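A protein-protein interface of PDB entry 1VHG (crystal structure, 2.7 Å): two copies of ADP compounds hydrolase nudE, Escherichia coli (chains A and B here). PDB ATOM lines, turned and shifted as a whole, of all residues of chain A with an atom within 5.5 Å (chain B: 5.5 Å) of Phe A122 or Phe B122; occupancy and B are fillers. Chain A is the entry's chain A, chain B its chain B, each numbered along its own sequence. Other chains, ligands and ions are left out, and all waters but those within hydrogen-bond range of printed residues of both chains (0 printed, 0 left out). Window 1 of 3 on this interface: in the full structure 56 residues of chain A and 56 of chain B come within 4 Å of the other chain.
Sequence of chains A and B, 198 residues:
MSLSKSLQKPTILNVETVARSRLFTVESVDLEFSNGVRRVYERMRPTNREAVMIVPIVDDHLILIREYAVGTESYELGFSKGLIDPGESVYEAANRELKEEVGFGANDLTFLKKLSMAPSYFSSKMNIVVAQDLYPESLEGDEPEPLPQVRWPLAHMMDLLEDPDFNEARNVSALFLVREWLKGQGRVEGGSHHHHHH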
ATOM      1  N   PHE A  24      10.377 -12.275  25.439  1.00  0.00           N
ATOM      2  CA  PHE A  24      10.317 -11.744  24.094  1.00  0.00           C
ATOM      3  C   PHE A  24       9.567 -10.435  23.943  1.00  0.00           C
ATOM      4  O   PHE A  24       8.388 -10.318  24.268  1.00  0.00           O
ATOM      5  CB  PHE A  24       9.649 -12.781  23.176  1.00  0.00           C
ATOM      6  CG  PHE A  24      10.458 -14.017  22.943  1.00  0.00           C
ATOM      7  CD1 PHE A  24      11.497 -14.019  22.037  1.00  0.00           C
ATOM      8  CD2 PHE A  24      10.170 -15.184  23.626  1.00  0.00           C
ATOM      9  CE1 PHE A  24      12.234 -15.166  21.813  1.00  0.00           C
ATOM     10  CE2 PHE A  24      10.900 -16.335  23.410  1.00  0.00           C
ATOM     11  CZ  PHE A  24      11.935 -16.327  22.499  1.00  0.00           C
ATOM     12  N   MET A  44      12.878  -8.206  16.862  1.00  0.00           N
ATOM     13  CA  MET A  44      13.011  -8.429  18.298  1.00  0.00           C
ATOM     14  C   MET A  44      13.628  -7.150  18.877  1.00  0.00           C
ATOM     15  O   MET A  44      14.532  -6.588  18.244  1.00  0.00           O
ATOM     16  CB  MET A  44      13.944  -9.602  18.585  1.00  0.00           C
ATOM     17  CG  MET A  44      13.306 -10.630  19.518  1.00  0.00           C
ATOM     18  SD  MET A  44      11.717 -11.335  18.723  1.00  0.00           S
ATOM     19  CE  MET A  44      10.473 -11.169  20.147  1.00  0.00           C
ATOM     20  N   GLY A  71      12.201 -25.475  21.641  1.00  0.00           N
ATOM     21  CA  GLY A  71      11.789 -25.106  20.292  1.00  0.00           C
ATOM     22  C   GLY A  71      11.594 -26.347  19.421  1.00  0.00           C
ATOM     23  O   GLY A  71      10.622 -26.380  18.664  1.00  0.00           O
ATOM     24  N   THR A  72      12.454 -27.345  19.494  1.00  0.00           N
ATOM     25  CA  THR A  72      12.350 -28.555  18.719  1.00  0.00           C
ATOM     26  C   THR A  72      11.944 -29.775  19.556  1.00  0.00           C
ATOM     27  O   THR A  72      11.934 -30.906  19.046  1.00  0.00           O
ATOM     28  CB  THR A  72      13.702 -28.954  18.074  1.00  0.00           C
ATOM     29  OG1 THR A  72      14.690 -29.067  19.114  1.00  0.00           O
ATOM     30  CG2 THR A  72      14.165 -27.976  17.040  1.00  0.00           C
ATOM     31  N   MET A 117      23.494 -13.314  14.535  1.00  0.00           N
ATOM     32  CA  MET A 117      22.597 -14.416  14.189  1.00  0.00           C
ATOM     33  C   MET A 117      21.288 -13.858  13.624  1.00  0.00           C
ATOM     34  O   MET A 117      20.455 -13.342  14.367  1.00  0.00           O
ATOM     35  CB  MET A 117      22.304 -15.357  15.334  1.00  0.00           C
ATOM     36  CG  MET A 117      23.459 -16.076  16.002  1.00  0.00           C
ATOM     37  SD  MET A 117      23.873 -15.351  17.722  1.00  0.00           S
ATOM     38  CE  MET A 117      23.125 -16.653  18.884  1.00  0.00           C
ATOM     39  N   ALA A 118      21.134 -13.941  12.309  1.00  0.00           N
ATOM     40  CA  ALA A 118      19.926 -13.448  11.641  1.00  0.00           C
ATOM     41  C   ALA A 118      19.628 -12.029  12.102  1.00  0.00           C
ATOM     42  O   ALA A 118      18.695 -11.763  12.859  1.00  0.00           O
ATOM     43  CB  ALA A 118      18.770 -14.390  11.897  1.00  0.00           C
ATOM     44  N   PRO A 119      20.435 -11.085  11.606  1.00  0.00           N
ATOM     45  CA  PRO A 119      20.331  -9.691  11.950  1.00  0.00           C
ATOM     46  C   PRO A 119      19.076  -9.009  11.466  1.00  0.00           C
ATOM     47  O   PRO A 119      18.853  -7.865  11.871  1.00  0.00           O
ATOM     48  CB  PRO A 119      21.587  -9.034  11.415  1.00  0.00           C
ATOM     49  CG  PRO A 119      22.416 -10.092  10.831  1.00  0.00           C
ATOM     50  CD  PRO A 119      21.582 -11.328  10.702  1.00  0.00           C
ATOM     51  N   SER A 120      18.276  -9.629  10.617  1.00  0.00           N
ATOM     52  CA  SER A 120      17.027  -9.063  10.140  1.00  0.00           C
ATOM     53  C   SER A 120      16.072  -8.844  11.317  1.00  0.00           C
ATOM     54  O   SER A 120      15.503  -7.775  11.445  1.00  0.00           O
ATOM     55  CB  SER A 120      16.312  -9.986   9.156  1.00  0.00           C
ATOM     56  OG  SER A 120      16.696  -9.728   7.826  1.00  0.00           O
ATOM     57  N   TYR A 121      15.951  -9.866  12.157  1.00  0.00           N
ATOM     58  CA  TYR A 121      15.101  -9.854  13.314  1.00  0.00           C
ATOM     59  C   TYR A 121      15.832  -9.744  14.638  1.00  0.00           C
ATOM     60  O   TYR A 121      15.238  -9.227  15.587  1.00  0.00           O
ATOM     61  CB  TYR A 121      14.252 -11.157  13.384  1.00  0.00           C
ATOM     62  CG  TYR A 121      13.665 -11.490  12.028  1.00  0.00           C
ATOM     63  CD1 TYR A 121      12.722 -10.642  11.451  1.00  0.00           C
ATOM     64  CD2 TYR A 121      14.092 -12.598  11.314  1.00  0.00           C
ATOM     65  CE1 TYR A 121      12.204 -10.903  10.201  1.00  0.00           C
ATOM     66  CE2 TYR A 121      13.572 -12.862  10.059  1.00  0.00           C
ATOM     67  CZ  TYR A 121      12.631 -12.015   9.512  1.00  0.00           C
ATOM     68  OH  TYR A 121      12.102 -12.276   8.261  1.00  0.00           O
ATOM     69  N   PHE A 122      17.024 -10.309  14.752  1.00  0.00           N
ATOM     70  CA  PHE A 122      17.714 -10.270  16.051  1.00  0.00           C
ATOM     71  C   PHE A 122      18.959  -9.410  15.983  1.00  0.00           C
ATOM     72  O   PHE A 122      19.474  -9.136  14.895  1.00  0.00           O
ATOM     73  CB  PHE A 122      18.032 -11.689  16.556  1.00  0.00           C
ATOM     74  CG  PHE A 122      16.966 -12.689  16.201  1.00  0.00           C
ATOM     75  CD1 PHE A 122      17.110 -13.485  15.073  1.00  0.00           C
ATOM     76  CD2 PHE A 122      15.794 -12.787  16.935  1.00  0.00           C
ATOM     77  CE1 PHE A 122      16.116 -14.383  14.709  1.00  0.00           C
ATOM     78  CE2 PHE A 122      14.799 -13.680  16.578  1.00  0.00           C
ATOM     79  CZ  PHE A 122      14.960 -14.482  15.464  1.00  0.00           C
ATOM     80  N   SER A 123      19.439  -8.945  17.136  1.00  0.00           N
ATOM     81  CA  SER A 123      20.629  -8.093  17.108  1.00  0.00           C
ATOM     82  C   SER A 123      21.771  -8.730  17.891  1.00  0.00           C
ATOM     83  O   SER A 123      22.949  -8.521  17.566  1.00  0.00           O
ATOM     84  CB  SER A 123      20.306  -6.698  17.626  1.00  0.00           C
ATOM     85  OG  SER A 123      19.574  -6.751  18.835  1.00  0.00           O
ATOM     86  N   SER A 124      21.415  -9.590  18.845  1.00  0.00           N
ATOM     87  CA  SER A 124      22.405 -10.238  19.670  1.00  0.00           C
ATOM     88  C   SER A 124      23.578 -10.818  18.891  1.00  0.00           C
ATOM     89  O   SER A 124      23.455 -11.317  17.773  1.00  0.00           O
ATOM     90  CB  SER A 124      21.791 -11.344  20.549  1.00  0.00           C
ATOM     91  OG  SER A 124      22.733 -11.722  21.566  1.00  0.00           O
ATOM     92  N   PHE B  24       5.209 -12.690  14.576  1.00  0.00           N
ATOM     93  CA  PHE B  24       5.707 -13.521  15.666  1.00  0.00           C
ATOM     94  C   PHE B  24       4.600 -13.972  16.604  1.00  0.00           C
ATOM     95  O   PHE B  24       3.746 -13.178  16.976  1.00  0.00           O
ATOM     96  CB  PHE B  24       6.767 -12.777  16.479  1.00  0.00           C
ATOM     97  CG  PHE B  24       7.982 -12.362  15.708  1.00  0.00           C
ATOM     98  CD1 PHE B  24       9.072 -13.204  15.596  1.00  0.00           C
ATOM     99  CD2 PHE B  24       8.033 -11.123  15.092  1.00  0.00           C
ATOM    100  CE1 PHE B  24      10.188 -12.826  14.889  1.00  0.00           C
ATOM    101  CE2 PHE B  24       9.153 -10.737  14.379  1.00  0.00           C
ATOM    102  CZ  PHE B  24      10.233 -11.591  14.280  1.00  0.00           C
ATOM    103  N   MET B  44       9.159 -19.796  20.079  1.00  0.00           N
ATOM    104  CA  MET B  44       8.469 -19.326  18.879  1.00  0.00           C
ATOM    105  C   MET B  44       7.560 -20.478  18.459  1.00  0.00           C
ATOM    106  O   MET B  44       8.026 -21.628  18.513  1.00  0.00           O
ATOM    107  CB  MET B  44       9.520 -19.036  17.807  1.00  0.00           C
ATOM    108  CG  MET B  44       9.349 -17.677  17.148  1.00  0.00           C
ATOM    109  SD  MET B  44       9.002 -16.330  18.473  1.00  0.00           S
ATOM    110  CE  MET B  44      10.766 -15.637  18.711  1.00  0.00           C
ATOM    111  N   GLY B  71      16.912  -5.641  12.127  1.00  0.00           N
ATOM    112  CA  GLY B  71      17.340  -6.068  13.453  1.00  0.00           C
ATOM    113  C   GLY B  71      18.528  -5.250  13.943  1.00  0.00           C
ATOM    114  O   GLY B  71      18.483  -4.655  15.025  1.00  0.00           O
ATOM    115  N   THR B  72      19.598  -5.188  13.187  1.00  0.00           N
ATOM    116  CA  THR B  72      20.803  -4.449  13.531  1.00  0.00           C
ATOM    117  C   THR B  72      20.848  -3.079  12.872  1.00  0.00           C
ATOM    118  O   THR B  72      21.820  -2.348  12.964  1.00  0.00           O
ATOM    119  CB  THR B  72      22.027  -5.264  13.030  1.00  0.00           C
ATOM    120  OG1 THR B  72      21.898  -5.448  11.601  1.00  0.00           O
ATOM    121  CG2 THR B  72      22.012  -6.644  13.635  1.00  0.00           C
ATOM    122  N   MET B 117      18.095 -23.881  13.264  1.00  0.00           N
ATOM    123  CA  MET B 117      18.459 -22.495  13.654  1.00  0.00           C
ATOM    124  C   MET B 117      17.953 -22.222  15.059  1.00  0.00           C
ATOM    125  O   MET B 117      16.742 -22.196  15.258  1.00  0.00           O
ATOM    126  CB  MET B 117      17.938 -21.492  12.635  1.00  0.00           C
ATOM    127  CG  MET B 117      18.819 -21.253  11.420  1.00  0.00           C
ATOM    128  SD  MET B 117      17.872 -20.702   9.853  1.00  0.00           S
ATOM    129  CE  MET B 117      17.442 -18.896  10.247  1.00  0.00           C
ATOM    130  N   ALA B 118      18.858 -22.144  16.024  1.00  0.00           N
ATOM    131  CA  ALA B 118      18.525 -21.901  17.421  1.00  0.00           C
ATOM    132  C   ALA B 118      17.319 -22.694  17.912  1.00  0.00           C
ATOM    133  O   ALA B 118      16.262 -22.148  18.265  1.00  0.00           O
ATOM    134  CB  ALA B 118      18.320 -20.405  17.629  1.00  0.00           C
ATOM    135  N   PRO B 119      17.496 -24.011  18.093  1.00  0.00           N
ATOM    136  CA  PRO B 119      16.452 -24.914  18.506  1.00  0.00           C
ATOM    137  C   PRO B 119      15.828 -24.674  19.856  1.00  0.00           C
ATOM    138  O   PRO B 119      14.761 -25.240  20.138  1.00  0.00           O
ATOM    139  CB  PRO B 119      17.039 -26.311  18.386  1.00  0.00           C
ATOM    140  CG  PRO B 119      18.316 -26.174  17.674  1.00  0.00           C
ATOM    141  CD  PRO B 119      18.737 -24.742  17.731  1.00  0.00           C
ATOM    142  N   SER B 120      16.433 -23.902  20.739  1.00  0.00           N
ATOM    143  CA  SER B 120      15.851 -23.618  22.039  1.00  0.00           C
ATOM    144  C   SER B 120      14.580 -22.798  21.877  1.00  0.00           C
ATOM    145  O   SER B 120      13.620 -22.968  22.630  1.00  0.00           O
ATOM    146  CB  SER B 120      16.856 -22.919  22.942  1.00  0.00           C
ATOM    147  OG  SER B 120      17.727 -23.877  23.547  1.00  0.00           O
ATOM    148  N   TYR B 121      14.560 -21.884  20.904  1.00  0.00           N
ATOM    149  CA  TYR B 121      13.381 -21.074  20.663  1.00  0.00           C
ATOM    150  C   TYR B 121      12.791 -21.316  19.281  1.00  0.00           C
ATOM    151  O   TYR B 121      11.641 -20.926  19.068  1.00  0.00           O
ATOM    152  CB  TYR B 121      13.649 -19.575  20.820  1.00  0.00           C
ATOM    153  CG  TYR B 121      14.581 -19.219  21.952  1.00  0.00           C
ATOM    154  CD1 TYR B 121      14.168 -19.305  23.274  1.00  0.00           C
ATOM    155  CD2 TYR B 121      15.887 -18.823  21.696  1.00  0.00           C
ATOM    156  CE1 TYR B 121      15.031 -18.994  24.310  1.00  0.00           C
ATOM    157  CE2 TYR B 121      16.754 -18.503  22.725  1.00  0.00           C
ATOM    158  CZ  TYR B 121      16.323 -18.593  24.032  1.00  0.00           C
ATOM    159  OH  TYR B 121      17.189 -18.285  25.060  1.00  0.00           O
ATOM    160  N   PHE B 122      13.544 -21.844  18.322  1.00  0.00           N
ATOM    161  CA  PHE B 122      13.004 -22.036  16.978  1.00  0.00           C
ATOM    162  C   PHE B 122      13.015 -23.481  16.525  1.00  0.00           C
ATOM    163  O   PHE B 122      13.666 -24.320  17.138  1.00  0.00           O
ATOM    164  CB  PHE B 122      13.773 -21.186  15.939  1.00  0.00           C
ATOM    165  CG  PHE B 122      13.853 -19.752  16.377  1.00  0.00           C
ATOM    166  CD1 PHE B 122      14.947 -19.291  17.089  1.00  0.00           C
ATOM    167  CD2 PHE B 122      12.786 -18.902  16.144  1.00  0.00           C
ATOM    168  CE1 PHE B 122      14.987 -17.979  17.539  1.00  0.00           C
ATOM    169  CE2 PHE B 122      12.825 -17.591  16.588  1.00  0.00           C
ATOM    170  CZ  PHE B 122      13.925 -17.131  17.290  1.00  0.00           C
ATOM    171  N   SER B 123      12.311 -23.757  15.430  1.00  0.00           N
ATOM    172  CA  SER B 123      12.271 -25.129  14.916  1.00  0.00           C
ATOM    173  C   SER B 123      12.408 -25.084  13.390  1.00  0.00           C
ATOM    174  O   SER B 123      12.107 -26.020  12.647  1.00  0.00           O
ATOM    175  CB  SER B 123      10.972 -25.811  15.324  1.00  0.00           C
ATOM    176  OG  SER B 123       9.929 -25.316  14.497  1.00  0.00           O
ATOM    177  N   SER B 124      12.916 -23.947  12.939  1.00  0.00           N
ATOM    178  CA  SER B 124      13.143 -23.673  11.539  1.00  0.00           C
ATOM    179  C   SER B 124      14.376 -24.390  10.995  1.00  0.00           C
ATOM    180  O   SER B 124      15.392 -24.548  11.668  1.00  0.00           O
ATOM    181  CB  SER B 124      13.304 -22.147  11.402  1.00  0.00           C
ATOM    182  OG  SER B 124      12.726 -21.657  10.214  1.00  0.00           O
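N of Thr A72 sits at hydrogen-bond distance from O of Pro B119, at 3.2 Å. The backbone carbonyl oxygen (O) of Ser A120 lies within hydrogen-bond range of the backbone NH (N) of Gly B71. The backbone carbonyl oxygen of Ser B120 sits at hydrogen-bond distance from the backbone NH of Gly A71, at 3.0 Å. The backbone NH (N) of Gly A71 lies within hydrogen-bond range of the backbone carbonyl oxygen (O) of Pro B119, 3.0 Å away. The backbone NH (N) of Thr B72 is in hydrogen-bond range of the backbone carbonyl oxygen (O) of Pro A119 (3.1 Å). The backbone NH (N) of Gly B71 sits close to the backbone carbonyl oxygen (O) of Pro A119 (3.0 Å).
N of Met B44 sits at hydrogen-bond distance from O of Tyr B121, at 2.9 Å. The backbone NH (N) of Met A44 sits at hydrogen-bond distance from the backbone carbonyl oxygen (O) of Tyr A121 (2.9 Å).
Among the printed residues, pairs that only touch across the chains: Phe A24 with Met B44 (3.5 Å), Phe A24 with Tyr B121 (3.8 Å), Gly A71 with Phe B122 (3.7 Å), Gly A71 with Ser B123 (3.4 Å), Thr A72 with Phe B122 (3.7 Å), Tyr A121 with Phe B24 (3.9 Å), Phe A122 with Thr B72 (3.8 Å), Phe A122 with Phe B122 (3.4 Å) and Ser A123 with Gly B71 (3.8 Å).
Met A117 touches none of the printed residues of chain B. Printed residues of chain B within 4 Å of Pro A119: Gly B71 (2.8 Å) and Thr B72 (3.1 Å). Of the printed residues of chain B, Ser A120 touches Gly B71. Printed residues of chain B within 4 Å of Phe A122: Thr B72 (3.8 Å) and Phe B122 (3.4 Å). Of the printed residues of chain B, Ser A123 touches Gly B71 (3.8 Å). Of the printed residues of chain A, Phe B24 touches Tyr A121 (3.9 Å). Met B117 touches none of the printed residues of chain A. Printed residues of chain A within 4 Å of Ser B120: Gly A71 (3.0 Å). Phe B122 touches three residues of chain A. The nearest printed residue of chain A that does not touch Ser B120 is Thr A72 (5.4 Å).
Printed residues of chain A that touch a printed residue of chain B: Phe A24, Gly A71, Thr A72, Pro A119, Ser A120, Tyr A121, Phe A122 and Ser A123. Of the 12 printed residues of chain B, 9 touch a printed residue of chain A. Hydrophobic or aromatic side chains of chain B that line the printed part of chain A: Phe B24, Met B44, Pro B119, Tyr B121 and Phe B122. Among the printed residues, no Asp or Glu carboxylate lies within 4 Å of a Lys or Arg side-chain nitrogen of the other chain.
Phe A24 touches Met B44, but with the chains exchanged Met A44 does not touch Phe B24 (4.4 Å). Phe A24 touches Tyr B121, and with the chains exchanged Tyr A121 touches Phe B24. Gly A71 touches Phe B122, but with the chains exchanged Phe A122 does not touch Gly B71 (4.01 Å). Thr A72 touches Pro B119, and with the chains exchanged Pro A119 touches Thr B72. Positions printed for both chains: 24, 44, 71, 72, 117, 118, 119, 120, 121, 122, 123 and 124. Of the 15 pairs that touch across the chains among the printed residues, 13 have their exchanged pair printed and touching as well.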
